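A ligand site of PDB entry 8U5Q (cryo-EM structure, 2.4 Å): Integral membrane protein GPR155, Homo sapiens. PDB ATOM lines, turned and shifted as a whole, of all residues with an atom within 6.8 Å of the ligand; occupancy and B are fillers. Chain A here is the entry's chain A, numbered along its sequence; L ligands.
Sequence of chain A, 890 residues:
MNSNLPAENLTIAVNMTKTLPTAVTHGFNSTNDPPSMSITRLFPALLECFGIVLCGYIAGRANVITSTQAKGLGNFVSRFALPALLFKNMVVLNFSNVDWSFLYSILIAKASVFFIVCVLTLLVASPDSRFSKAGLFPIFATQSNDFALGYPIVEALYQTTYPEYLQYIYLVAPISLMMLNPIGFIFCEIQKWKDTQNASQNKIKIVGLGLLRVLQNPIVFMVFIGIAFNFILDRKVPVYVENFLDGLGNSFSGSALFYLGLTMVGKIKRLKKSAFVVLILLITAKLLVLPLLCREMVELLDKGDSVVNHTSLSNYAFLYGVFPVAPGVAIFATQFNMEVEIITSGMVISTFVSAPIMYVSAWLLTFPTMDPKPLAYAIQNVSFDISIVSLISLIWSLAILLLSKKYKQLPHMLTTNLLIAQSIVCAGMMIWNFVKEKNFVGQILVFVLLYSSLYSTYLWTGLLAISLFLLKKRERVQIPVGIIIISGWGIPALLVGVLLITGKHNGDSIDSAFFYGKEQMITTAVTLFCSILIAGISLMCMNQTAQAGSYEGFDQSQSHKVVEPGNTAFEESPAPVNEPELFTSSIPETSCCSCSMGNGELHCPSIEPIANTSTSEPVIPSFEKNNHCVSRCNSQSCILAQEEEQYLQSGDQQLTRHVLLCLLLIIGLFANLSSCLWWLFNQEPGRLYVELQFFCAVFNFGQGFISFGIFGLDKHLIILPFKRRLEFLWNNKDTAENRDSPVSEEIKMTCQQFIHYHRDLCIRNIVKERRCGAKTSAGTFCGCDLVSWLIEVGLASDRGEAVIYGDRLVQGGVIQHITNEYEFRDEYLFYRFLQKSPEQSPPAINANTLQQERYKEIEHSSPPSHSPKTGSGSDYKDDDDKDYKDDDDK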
ATOM      1  N   GLY A  74      14.452 -15.882 -11.754  1.00  0.00           N
ATOM      2  CA  GLY A  74      13.970 -15.071 -10.649  1.00  0.00           C
ATOM      3  C   GLY A  74      12.530 -15.350 -10.288  1.00  0.00           C
ATOM      4  O   GLY A  74      12.190 -15.443  -9.105  1.00  0.00           O
ATOM      5  N   VAL A  77      12.399 -18.787  -8.649  1.00  0.00           N
ATOM      6  CA  VAL A  77      12.904 -18.715  -7.282  1.00  0.00           C
ATOM      7  C   VAL A  77      11.891 -18.028  -6.367  1.00  0.00           C
ATOM      8  O   VAL A  77      11.512 -18.566  -5.321  1.00  0.00           O
ATOM      9  CB  VAL A  77      14.262 -17.983  -7.268  1.00  0.00           C
ATOM     10  CG1 VAL A  77      14.623 -17.527  -5.889  1.00  0.00           C
ATOM     11  CG2 VAL A  77      15.332 -18.891  -7.835  1.00  0.00           C
ATOM     12  N   SER A  78      11.421 -16.848  -6.764  1.00  0.00           N
ATOM     13  CA  SER A  78      10.611 -16.038  -5.863  1.00  0.00           C
ATOM     14  C   SER A  78       9.182 -16.549  -5.756  1.00  0.00           C
ATOM     15  O   SER A  78       8.573 -16.460  -4.678  1.00  0.00           O
ATOM     16  CB  SER A  78      10.634 -14.577  -6.304  1.00  0.00           C
ATOM     17  OG  SER A  78      10.162 -14.433  -7.632  1.00  0.00           O
ATOM     18  N   LEU A  82      10.923 -20.508  -3.399  1.00  0.00           N
ATOM     19  CA  LEU A  82      10.956 -19.883  -2.070  1.00  0.00           C
ATOM     20  C   LEU A  82       9.653 -20.101  -1.312  1.00  0.00           C
ATOM     21  O   LEU A  82       9.723 -20.529  -0.141  1.00  0.00           O
ATOM     22  CB  LEU A  82      11.299 -18.395  -2.199  1.00  0.00           C
ATOM     23  CG  LEU A  82      11.296 -17.559  -0.930  1.00  0.00           C
ATOM     24  CD1 LEU A  82      12.255 -18.127   0.097  1.00  0.00           C
ATOM     25  CD2 LEU A  82      11.677 -16.126  -1.269  1.00  0.00           C
ATOM     26  N   GLN A 143      17.380  -5.867   6.641  1.00  0.00           N
ATOM     27  CA  GLN A 143      16.871  -7.058   5.969  1.00  0.00           C
ATOM     28  C   GLN A 143      18.027  -7.897   5.432  1.00  0.00           C
ATOM     29  O   GLN A 143      18.828  -7.432   4.612  1.00  0.00           O
ATOM     30  CB  GLN A 143      15.925  -6.659   4.840  1.00  0.00           C
ATOM     31  CG  GLN A 143      15.070  -7.809   4.349  1.00  0.00           C
ATOM     32  CD  GLN A 143      14.106  -7.408   3.253  1.00  0.00           C
ATOM     33  OE1 GLN A 143      13.617  -6.279   3.224  1.00  0.00           O
ATOM     34  NE2 GLN A 143      13.820  -8.332   2.350  1.00  0.00           N
ATOM     35  N   SER A 144      18.112  -9.152   5.887  1.00  0.00           N
ATOM     36  CA  SER A 144      19.204 -10.053   5.554  1.00  0.00           C
ATOM     37  C   SER A 144      18.861 -10.968   4.383  1.00  0.00           C
ATOM     38  O   SER A 144      17.691 -11.272   4.129  1.00  0.00           O
ATOM     39  CB  SER A 144      19.579 -10.919   6.752  1.00  0.00           C
ATOM     40  OG  SER A 144      20.177 -10.187   7.795  1.00  0.00           O
ATOM     41  N   ASN A 145      19.909 -11.414   3.693  1.00  0.00           N
ATOM     42  CA  ASN A 145      19.829 -12.472   2.692  1.00  0.00           C
ATOM     43  C   ASN A 145      19.726 -13.824   3.387  1.00  0.00           C
ATOM     44  O   ASN A 145      20.591 -14.695   3.282  1.00  0.00           O
ATOM     45  CB  ASN A 145      21.037 -12.379   1.773  1.00  0.00           C
ATOM     46  CG  ASN A 145      20.822 -13.071   0.449  1.00  0.00           C
ATOM     47  OD1 ASN A 145      20.344 -14.195   0.392  1.00  0.00           O
ATOM     48  ND2 ASN A 145      21.208 -12.409  -0.622  1.00  0.00           N
ATOM     49  N   ASP A 146      18.620 -14.000   4.113  1.00  0.00           N
ATOM     50  CA  ASP A 146      18.499 -15.085   5.082  1.00  0.00           C
ATOM     51  C   ASP A 146      18.379 -16.442   4.420  1.00  0.00           C
ATOM     52  O   ASP A 146      18.971 -17.422   4.892  1.00  0.00           O
ATOM     53  CB  ASP A 146      17.281 -14.831   5.963  1.00  0.00           C
ATOM     54  CG  ASP A 146      17.472 -13.663   6.877  1.00  0.00           C
ATOM     55  OD1 ASP A 146      18.473 -13.667   7.600  1.00  0.00           O
ATOM     56  OD2 ASP A 146      16.638 -12.732   6.852  1.00  0.00           O
ATOM     57  N   PHE A 147      17.588 -16.535   3.357  1.00  0.00           N
ATOM     58  CA  PHE A 147      17.235 -17.837   2.823  1.00  0.00           C
ATOM     59  C   PHE A 147      18.280 -18.338   1.837  1.00  0.00           C
ATOM     60  O   PHE A 147      18.723 -19.490   1.937  1.00  0.00           O
ATOM     61  CB  PHE A 147      15.849 -17.767   2.189  1.00  0.00           C
ATOM     62  CG  PHE A 147      14.794 -17.273   3.130  1.00  0.00           C
ATOM     63  CD1 PHE A 147      14.394 -18.056   4.203  1.00  0.00           C
ATOM     64  CD2 PHE A 147      14.203 -16.032   2.965  1.00  0.00           C
ATOM     65  CE1 PHE A 147      13.435 -17.609   5.080  1.00  0.00           C
ATOM     66  CE2 PHE A 147      13.244 -15.586   3.841  1.00  0.00           C
ATOM     67  CZ  PHE A 147      12.852 -16.381   4.901  1.00  0.00           C
ATOM     68  N   ALA A 148      18.708 -17.498   0.906  1.00  0.00           N
ATOM     69  CA  ALA A 148      19.683 -17.936  -0.090  1.00  0.00           C
ATOM     70  C   ALA A 148      21.069 -18.106   0.534  1.00  0.00           C
ATOM     71  O   ALA A 148      21.688 -19.159   0.386  1.00  0.00           O
ATOM     72  CB  ALA A 148      19.728 -16.953  -1.260  1.00  0.00           C
ATOM     73  N   LEU A 149      21.559 -17.091   1.243  1.00  0.00           N
ATOM     74  CA  LEU A 149      22.902 -17.160   1.805  1.00  0.00           C
ATOM     75  C   LEU A 149      22.916 -17.550   3.269  1.00  0.00           C
ATOM     76  O   LEU A 149      23.789 -18.315   3.684  1.00  0.00           O
ATOM     77  CB  LEU A 149      23.621 -15.808   1.620  1.00  0.00           C
ATOM     78  CG  LEU A 149      24.131 -15.579   0.195  1.00  0.00           C
ATOM     79  CD1 LEU A 149      24.455 -14.144  -0.075  1.00  0.00           C
ATOM     80  CD2 LEU A 149      25.347 -16.393  -0.045  1.00  0.00           C
ATOM     81  N   GLY A 150      21.970 -17.072   4.063  1.00  0.00           N
ATOM     82  CA  GLY A 150      21.995 -17.367   5.487  1.00  0.00           C
ATOM     83  C   GLY A 150      21.788 -18.836   5.797  1.00  0.00           C
ATOM     84  O   GLY A 150      22.475 -19.396   6.658  1.00  0.00           O
ATOM     85  N   ASN A 217       4.158  -9.801  -0.182  1.00  0.00           N
ATOM     86  CA  ASN A 217       5.430 -10.486  -0.303  1.00  0.00           C
ATOM     87  C   ASN A 217       5.237 -11.977  -0.084  1.00  0.00           C
ATOM     88  O   ASN A 217       4.584 -12.363   0.899  1.00  0.00           O
ATOM     89  CB  ASN A 217       6.429  -9.903   0.696  1.00  0.00           C
ATOM     90  CG  ASN A 217       7.842 -10.351   0.445  1.00  0.00           C
ATOM     91  OD1 ASN A 217       8.138 -11.541   0.406  1.00  0.00           O
ATOM     92  ND2 ASN A 217       8.737  -9.385   0.266  1.00  0.00           N
ATOM     93  N   ILE A 219       7.174 -14.162   1.079  1.00  0.00           N
ATOM     94  CA  ILE A 219       7.731 -14.540   2.366  1.00  0.00           C
ATOM     95  C   ILE A 219       6.694 -14.361   3.469  1.00  0.00           C
ATOM     96  O   ILE A 219       6.505 -15.236   4.317  1.00  0.00           O
ATOM     97  CB  ILE A 219       9.013 -13.736   2.642  1.00  0.00           C
ATOM     98  CG1 ILE A 219      10.065 -14.068   1.575  1.00  0.00           C
ATOM     99  CG2 ILE A 219       9.557 -14.039   4.014  1.00  0.00           C
ATOM    100  CD1 ILE A 219      11.197 -13.089   1.521  1.00  0.00           C
ATOM    101  N   PHE A 252      15.481 -24.206  -4.174  1.00  0.00           N
ATOM    102  CA  PHE A 252      15.632 -22.786  -3.913  1.00  0.00           C
ATOM    103  C   PHE A 252      17.094 -22.401  -3.703  1.00  0.00           C
ATOM    104  O   PHE A 252      17.571 -21.424  -4.301  1.00  0.00           O
ATOM    105  CB  PHE A 252      14.805 -22.345  -2.700  1.00  0.00           C
ATOM    106  CG  PHE A 252      15.072 -20.923  -2.284  1.00  0.00           C
ATOM    107  CD1 PHE A 252      14.485 -19.874  -2.955  1.00  0.00           C
ATOM    108  CD2 PHE A 252      15.955 -20.647  -1.253  1.00  0.00           C
ATOM    109  CE1 PHE A 252      14.753 -18.568  -2.577  1.00  0.00           C
ATOM    110  CE2 PHE A 252      16.219 -19.352  -0.884  1.00  0.00           C
ATOM    111  CZ  PHE A 252      15.615 -18.317  -1.550  1.00  0.00           C
ATOM    112  N   SER A 255      19.344 -22.302  -6.859  1.00  0.00           N
ATOM    113  CA  SER A 255      18.720 -21.486  -7.884  1.00  0.00           C
ATOM    114  C   SER A 255      18.674 -20.026  -7.476  1.00  0.00           C
ATOM    115  O   SER A 255      18.842 -19.130  -8.313  1.00  0.00           O
ATOM    116  CB  SER A 255      17.313 -22.028  -8.153  1.00  0.00           C
ATOM    117  OG  SER A 255      16.688 -21.368  -9.238  1.00  0.00           O
ATOM    118  N   ALA A 256      18.470 -19.757  -6.186  1.00  0.00           N
ATOM    119  CA  ALA A 256      18.414 -18.389  -5.681  1.00  0.00           C
ATOM    120  C   ALA A 256      19.799 -17.760  -5.629  1.00  0.00           C
ATOM    121  O   ALA A 256      19.963 -16.578  -5.944  1.00  0.00           O
ATOM    122  CB  ALA A 256      17.781 -18.365  -4.300  1.00  0.00           C
ATOM    123  N   LEU A 257      20.805 -18.530  -5.207  1.00  0.00           N
ATOM    124  CA  LEU A 257      22.179 -18.047  -5.245  1.00  0.00           C
ATOM    125  C   LEU A 257      22.602 -17.717  -6.668  1.00  0.00           C
ATOM    126  O   LEU A 257      23.270 -16.711  -6.911  1.00  0.00           O
ATOM    127  CB  LEU A 257      23.106 -19.094  -4.634  1.00  0.00           C
ATOM    128  CG  LEU A 257      22.921 -19.337  -3.143  1.00  0.00           C
ATOM    129  CD1 LEU A 257      23.650 -20.591  -2.718  1.00  0.00           C
ATOM    130  CD2 LEU A 257      23.435 -18.140  -2.383  1.00  0.00           C
ATOM    131  N   PHE A 258      22.211 -18.557  -7.622  1.00  0.00           N
ATOM    132  CA  PHE A 258      22.558 -18.319  -9.015  1.00  0.00           C
ATOM    133  C   PHE A 258      21.833 -17.099  -9.569  1.00  0.00           C
ATOM    134  O   PHE A 258      22.411 -16.318 -10.326  1.00  0.00           O
ATOM    135  CB  PHE A 258      22.240 -19.560  -9.844  1.00  0.00           C
ATOM    136  CG  PHE A 258      22.838 -19.560 -11.208  1.00  0.00           C
ATOM    137  CD1 PHE A 258      22.188 -18.932 -12.262  1.00  0.00           C
ATOM    138  CD2 PHE A 258      24.027 -20.202 -11.464  1.00  0.00           C
ATOM    139  CE1 PHE A 258      22.731 -18.927 -13.514  1.00  0.00           C
ATOM    140  CE2 PHE A 258      24.573 -20.203 -12.722  1.00  0.00           C
ATOM    141  CZ  PHE A 258      23.914 -19.563 -13.748  1.00  0.00           C
ATOM    142  N   TYR A 259      20.559 -16.918  -9.207  1.00  0.00           N
ATOM    143  CA  TYR A 259      19.834 -15.723  -9.632  1.00  0.00           C
ATOM    144  C   TYR A 259      20.438 -14.479  -9.000  1.00  0.00           C
ATOM    145  O   TYR A 259      20.487 -13.415  -9.631  1.00  0.00           O
ATOM    146  CB  TYR A 259      18.354 -15.828  -9.281  1.00  0.00           C
ATOM    147  CG  TYR A 259      17.571 -14.620  -9.722  1.00  0.00           C
ATOM    148  CD1 TYR A 259      17.476 -14.296 -11.064  1.00  0.00           C
ATOM    149  CD2 TYR A 259      16.940 -13.795  -8.806  1.00  0.00           C
ATOM    150  CE1 TYR A 259      16.771 -13.200 -11.488  1.00  0.00           C
ATOM    151  CE2 TYR A 259      16.228 -12.687  -9.216  1.00  0.00           C
ATOM    152  CZ  TYR A 259      16.138 -12.399 -10.565  1.00  0.00           C
ATOM    153  OH  TYR A 259      15.442 -11.299 -10.987  1.00  0.00           O
ATOM    154  N   LEU A 260      20.874 -14.587  -7.742  1.00  0.00           N
ATOM    155  CA  LEU A 260      21.583 -13.491  -7.103  1.00  0.00           C
ATOM    156  C   LEU A 260      22.836 -13.119  -7.887  1.00  0.00           C
ATOM    157  O   LEU A 260      23.114 -11.937  -8.091  1.00  0.00           O
ATOM    158  CB  LEU A 260      21.907 -13.875  -5.660  1.00  0.00           C
ATOM    159  CG  LEU A 260      22.728 -12.927  -4.784  1.00  0.00           C
ATOM    160  CD1 LEU A 260      22.115 -11.549  -4.778  1.00  0.00           C
ATOM    161  CD2 LEU A 260      22.798 -13.497  -3.386  1.00  0.00           C
ATOM    162  N   THR A 263      21.712 -11.251 -11.065  1.00  0.00           N
ATOM    163  CA  THR A 263      21.243  -9.893 -10.822  1.00  0.00           C
ATOM    164  C   THR A 263      22.351  -8.961 -10.364  1.00  0.00           C
ATOM    165  O   THR A 263      22.185  -7.744 -10.440  1.00  0.00           O
ATOM    166  CB  THR A 263      20.110  -9.896  -9.796  1.00  0.00           C
ATOM    167  OG1 THR A 263      20.488 -10.672  -8.653  1.00  0.00           O
ATOM    168  CG2 THR A 263      18.866 -10.502 -10.405  1.00  0.00           C
ATOM    169  N   PRO A 324      24.235 -10.724   4.227  1.00  0.00           N
ATOM    170  CA  PRO A 324      24.171  -9.534   3.365  1.00  0.00           C
ATOM    171  C   PRO A 324      22.736  -9.031   3.219  1.00  0.00           C
ATOM    172  O   PRO A 324      21.780  -9.639   3.696  1.00  0.00           O
ATOM    173  CB  PRO A 324      24.728 -10.019   2.035  1.00  0.00           C
ATOM    174  CG  PRO A 324      24.576 -11.478   2.068  1.00  0.00           C
ATOM    175  CD  PRO A 324      24.700 -11.901   3.492  1.00  0.00           C
ATOM    176  N   VAL A 325      22.609  -7.897   2.540  1.00  0.00           N
ATOM    177  CA  VAL A 325      21.300  -7.304   2.338  1.00  0.00           C
ATOM    178  C   VAL A 325      20.467  -8.219   1.453  1.00  0.00           C
ATOM    179  O   VAL A 325      20.966  -8.824   0.505  1.00  0.00           O
ATOM    180  CB  VAL A 325      21.431  -5.898   1.727  1.00  0.00           C
ATOM    181  CG1 VAL A 325      20.068  -5.302   1.445  1.00  0.00           C
ATOM    182  CG2 VAL A 325      22.194  -5.001   2.679  1.00  0.00           C
ATOM    183  N   ALA A 326      19.187  -8.349   1.793  1.00  0.00           N
ATOM    184  CA  ALA A 326      18.297  -9.175   1.015  1.00  0.00           C
ATOM    185  C   ALA A 326      18.157  -8.612  -0.401  1.00  0.00           C
ATOM    186  O   ALA A 326      18.052  -7.398  -0.574  1.00  0.00           O
ATOM    187  CB  ALA A 326      16.930  -9.255   1.679  1.00  0.00           C
ATOM    188  N   PRO A 327      18.159  -9.467  -1.428  1.00  0.00           N
ATOM    189  CA  PRO A 327      17.918  -8.952  -2.783  1.00  0.00           C
ATOM    190  C   PRO A 327      16.548  -8.297  -2.915  1.00  0.00           C
ATOM    191  O   PRO A 327      16.359  -7.453  -3.790  1.00  0.00           O
ATOM    192  CB  PRO A 327      18.044 -10.209  -3.654  1.00  0.00           C
ATOM    193  CG  PRO A 327      18.810 -11.174  -2.824  1.00  0.00           C
ATOM    194  CD  PRO A 327      18.383 -10.916  -1.427  1.00  0.00           C
ATOM    195  N   GLY A 328      15.609  -8.664  -2.044  1.00  0.00           N
ATOM    196  CA  GLY A 328      14.294  -8.051  -2.075  1.00  0.00           C
ATOM    197  C   GLY A 328      14.310  -6.552  -1.864  1.00  0.00           C
ATOM    198  O   GLY A 328      13.421  -5.851  -2.346  1.00  0.00           O
ATOM    199  N   ILE A 331      14.690  -4.959  -5.031  1.00  0.00           N
ATOM    200  CA  ILE A 331      13.445  -5.096  -5.775  1.00  0.00           C
ATOM    201  C   ILE A 331      12.435  -4.054  -5.317  1.00  0.00           C
ATOM    202  O   ILE A 331      11.746  -3.448  -6.149  1.00  0.00           O
ATOM    203  CB  ILE A 331      12.915  -6.540  -5.632  1.00  0.00           C
ATOM    204  CG1 ILE A 331      13.848  -7.490  -6.386  1.00  0.00           C
ATOM    205  CG2 ILE A 331      11.502  -6.652  -6.166  1.00  0.00           C
ATOM    206  CD1 ILE A 331      13.657  -8.951  -6.059  1.00  0.00           C
HETATM  207  C1  LIG L   1      15.416 -14.004  -3.770  1.00  0.00           C
HETATM  208  C2  LIG L   1      16.017 -14.292  -2.574  1.00  0.00           C
HETATM  209  C3  LIG L   1      17.359 -14.710  -2.549  1.00  0.00           C
HETATM  210  C4  LIG L   1      18.066 -14.832  -3.733  1.00  0.00           C
HETATM  211  C5  LIG L   1      17.454 -14.541  -4.938  1.00  0.00           C
HETATM  212  C6  LIG L   1      16.134 -14.122  -4.967  1.00  0.00           C
HETATM  213  C7  LIG L   1      15.109 -14.087  -1.586  1.00  0.00           C
HETATM  214  C8  LIG L   1      13.932 -13.673  -2.172  1.00  0.00           C
HETATM  215  C9  LIG L   1      15.022 -14.210  -0.062  1.00  0.00           C
HETATM  216  C10 LIG L   1      16.317 -13.816   0.644  1.00  0.00           C
HETATM  217  N1  LIG L   1      14.131 -13.625  -3.514  1.00  0.00           N
HETATM  218  O1  LIG L   1      17.099 -14.693   1.099  1.00  0.00           O
HETATM  219  O2  LIG L   1      16.602 -12.591   0.808  1.00  0.00           O
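CG1 of Val 77 touches C6 of the ligand, at 3.8 Å.
Leu 82 touches the ligand.
O of Ser 144 touches O2 of the ligand (3.7 Å).
Ala 256 touches the ligand (O to C5, 3.4 Å).
Tyr 259 touches the ligand (CD2 to C6, 3.9 Å).
Ala 326 touches the ligand.
CD of Pro 327 touches O2 of the ligand, at 3.3 Å.
Hydrophobic or aromatic side chains that line the ligand: Val 77, Leu 82, Phe 147, Ala 148, Ala 256, Tyr 259, Ala 326 and Pro 327.
Within 4 Å of the ligand: Val 77, Leu 82, Ser 144, Asn 145, Asp 146, Phe 147, Ala 148, Ala 256, Tyr 259, Ala 326 and Pro 327.
The backbone NH of Asp 146 sits at hydrogen-bond distance from an oxygen (O1) of the ligand, 3.4 Å away.
N of Ala 148 is in hydrogen-bond range of O1 of the ligand (3.2 Å).
The backbone NH of Phe 147 is in hydrogen-bond range of an oxygen (O1) of the ligand (3.0 Å).
OD1 of Asn 145 sits close to O1 of the ligand (3.4 Å).
The backbone carbonyl oxygen (O) of Val 77 is in hydrogen-bond range of the backbone NH (N) of Leu 82, at 2.8 Å.
The backbone carbonyl oxygen (O) of Tyr 259 sits at hydrogen-bond distance from the side-chain hydroxyl (OG1) of Thr 263 (2.9 Å).
The side-chain amide oxygen (OD1) of Asn 145 lies within hydrogen-bond range of the backbone NH (N) of Leu 149 (3.3 Å).
N of Asn 145 sits at hydrogen-bond distance from O of Pro 324 (2.6 Å).
The backbone NH (N) of Gly 150 lies within hydrogen-bond range of the backbone carbonyl oxygen (O) of Asn 145, 2.9 Å away.
O of Gln 143 lies within hydrogen-bond range of N of Ala 326, 3.0 Å away.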
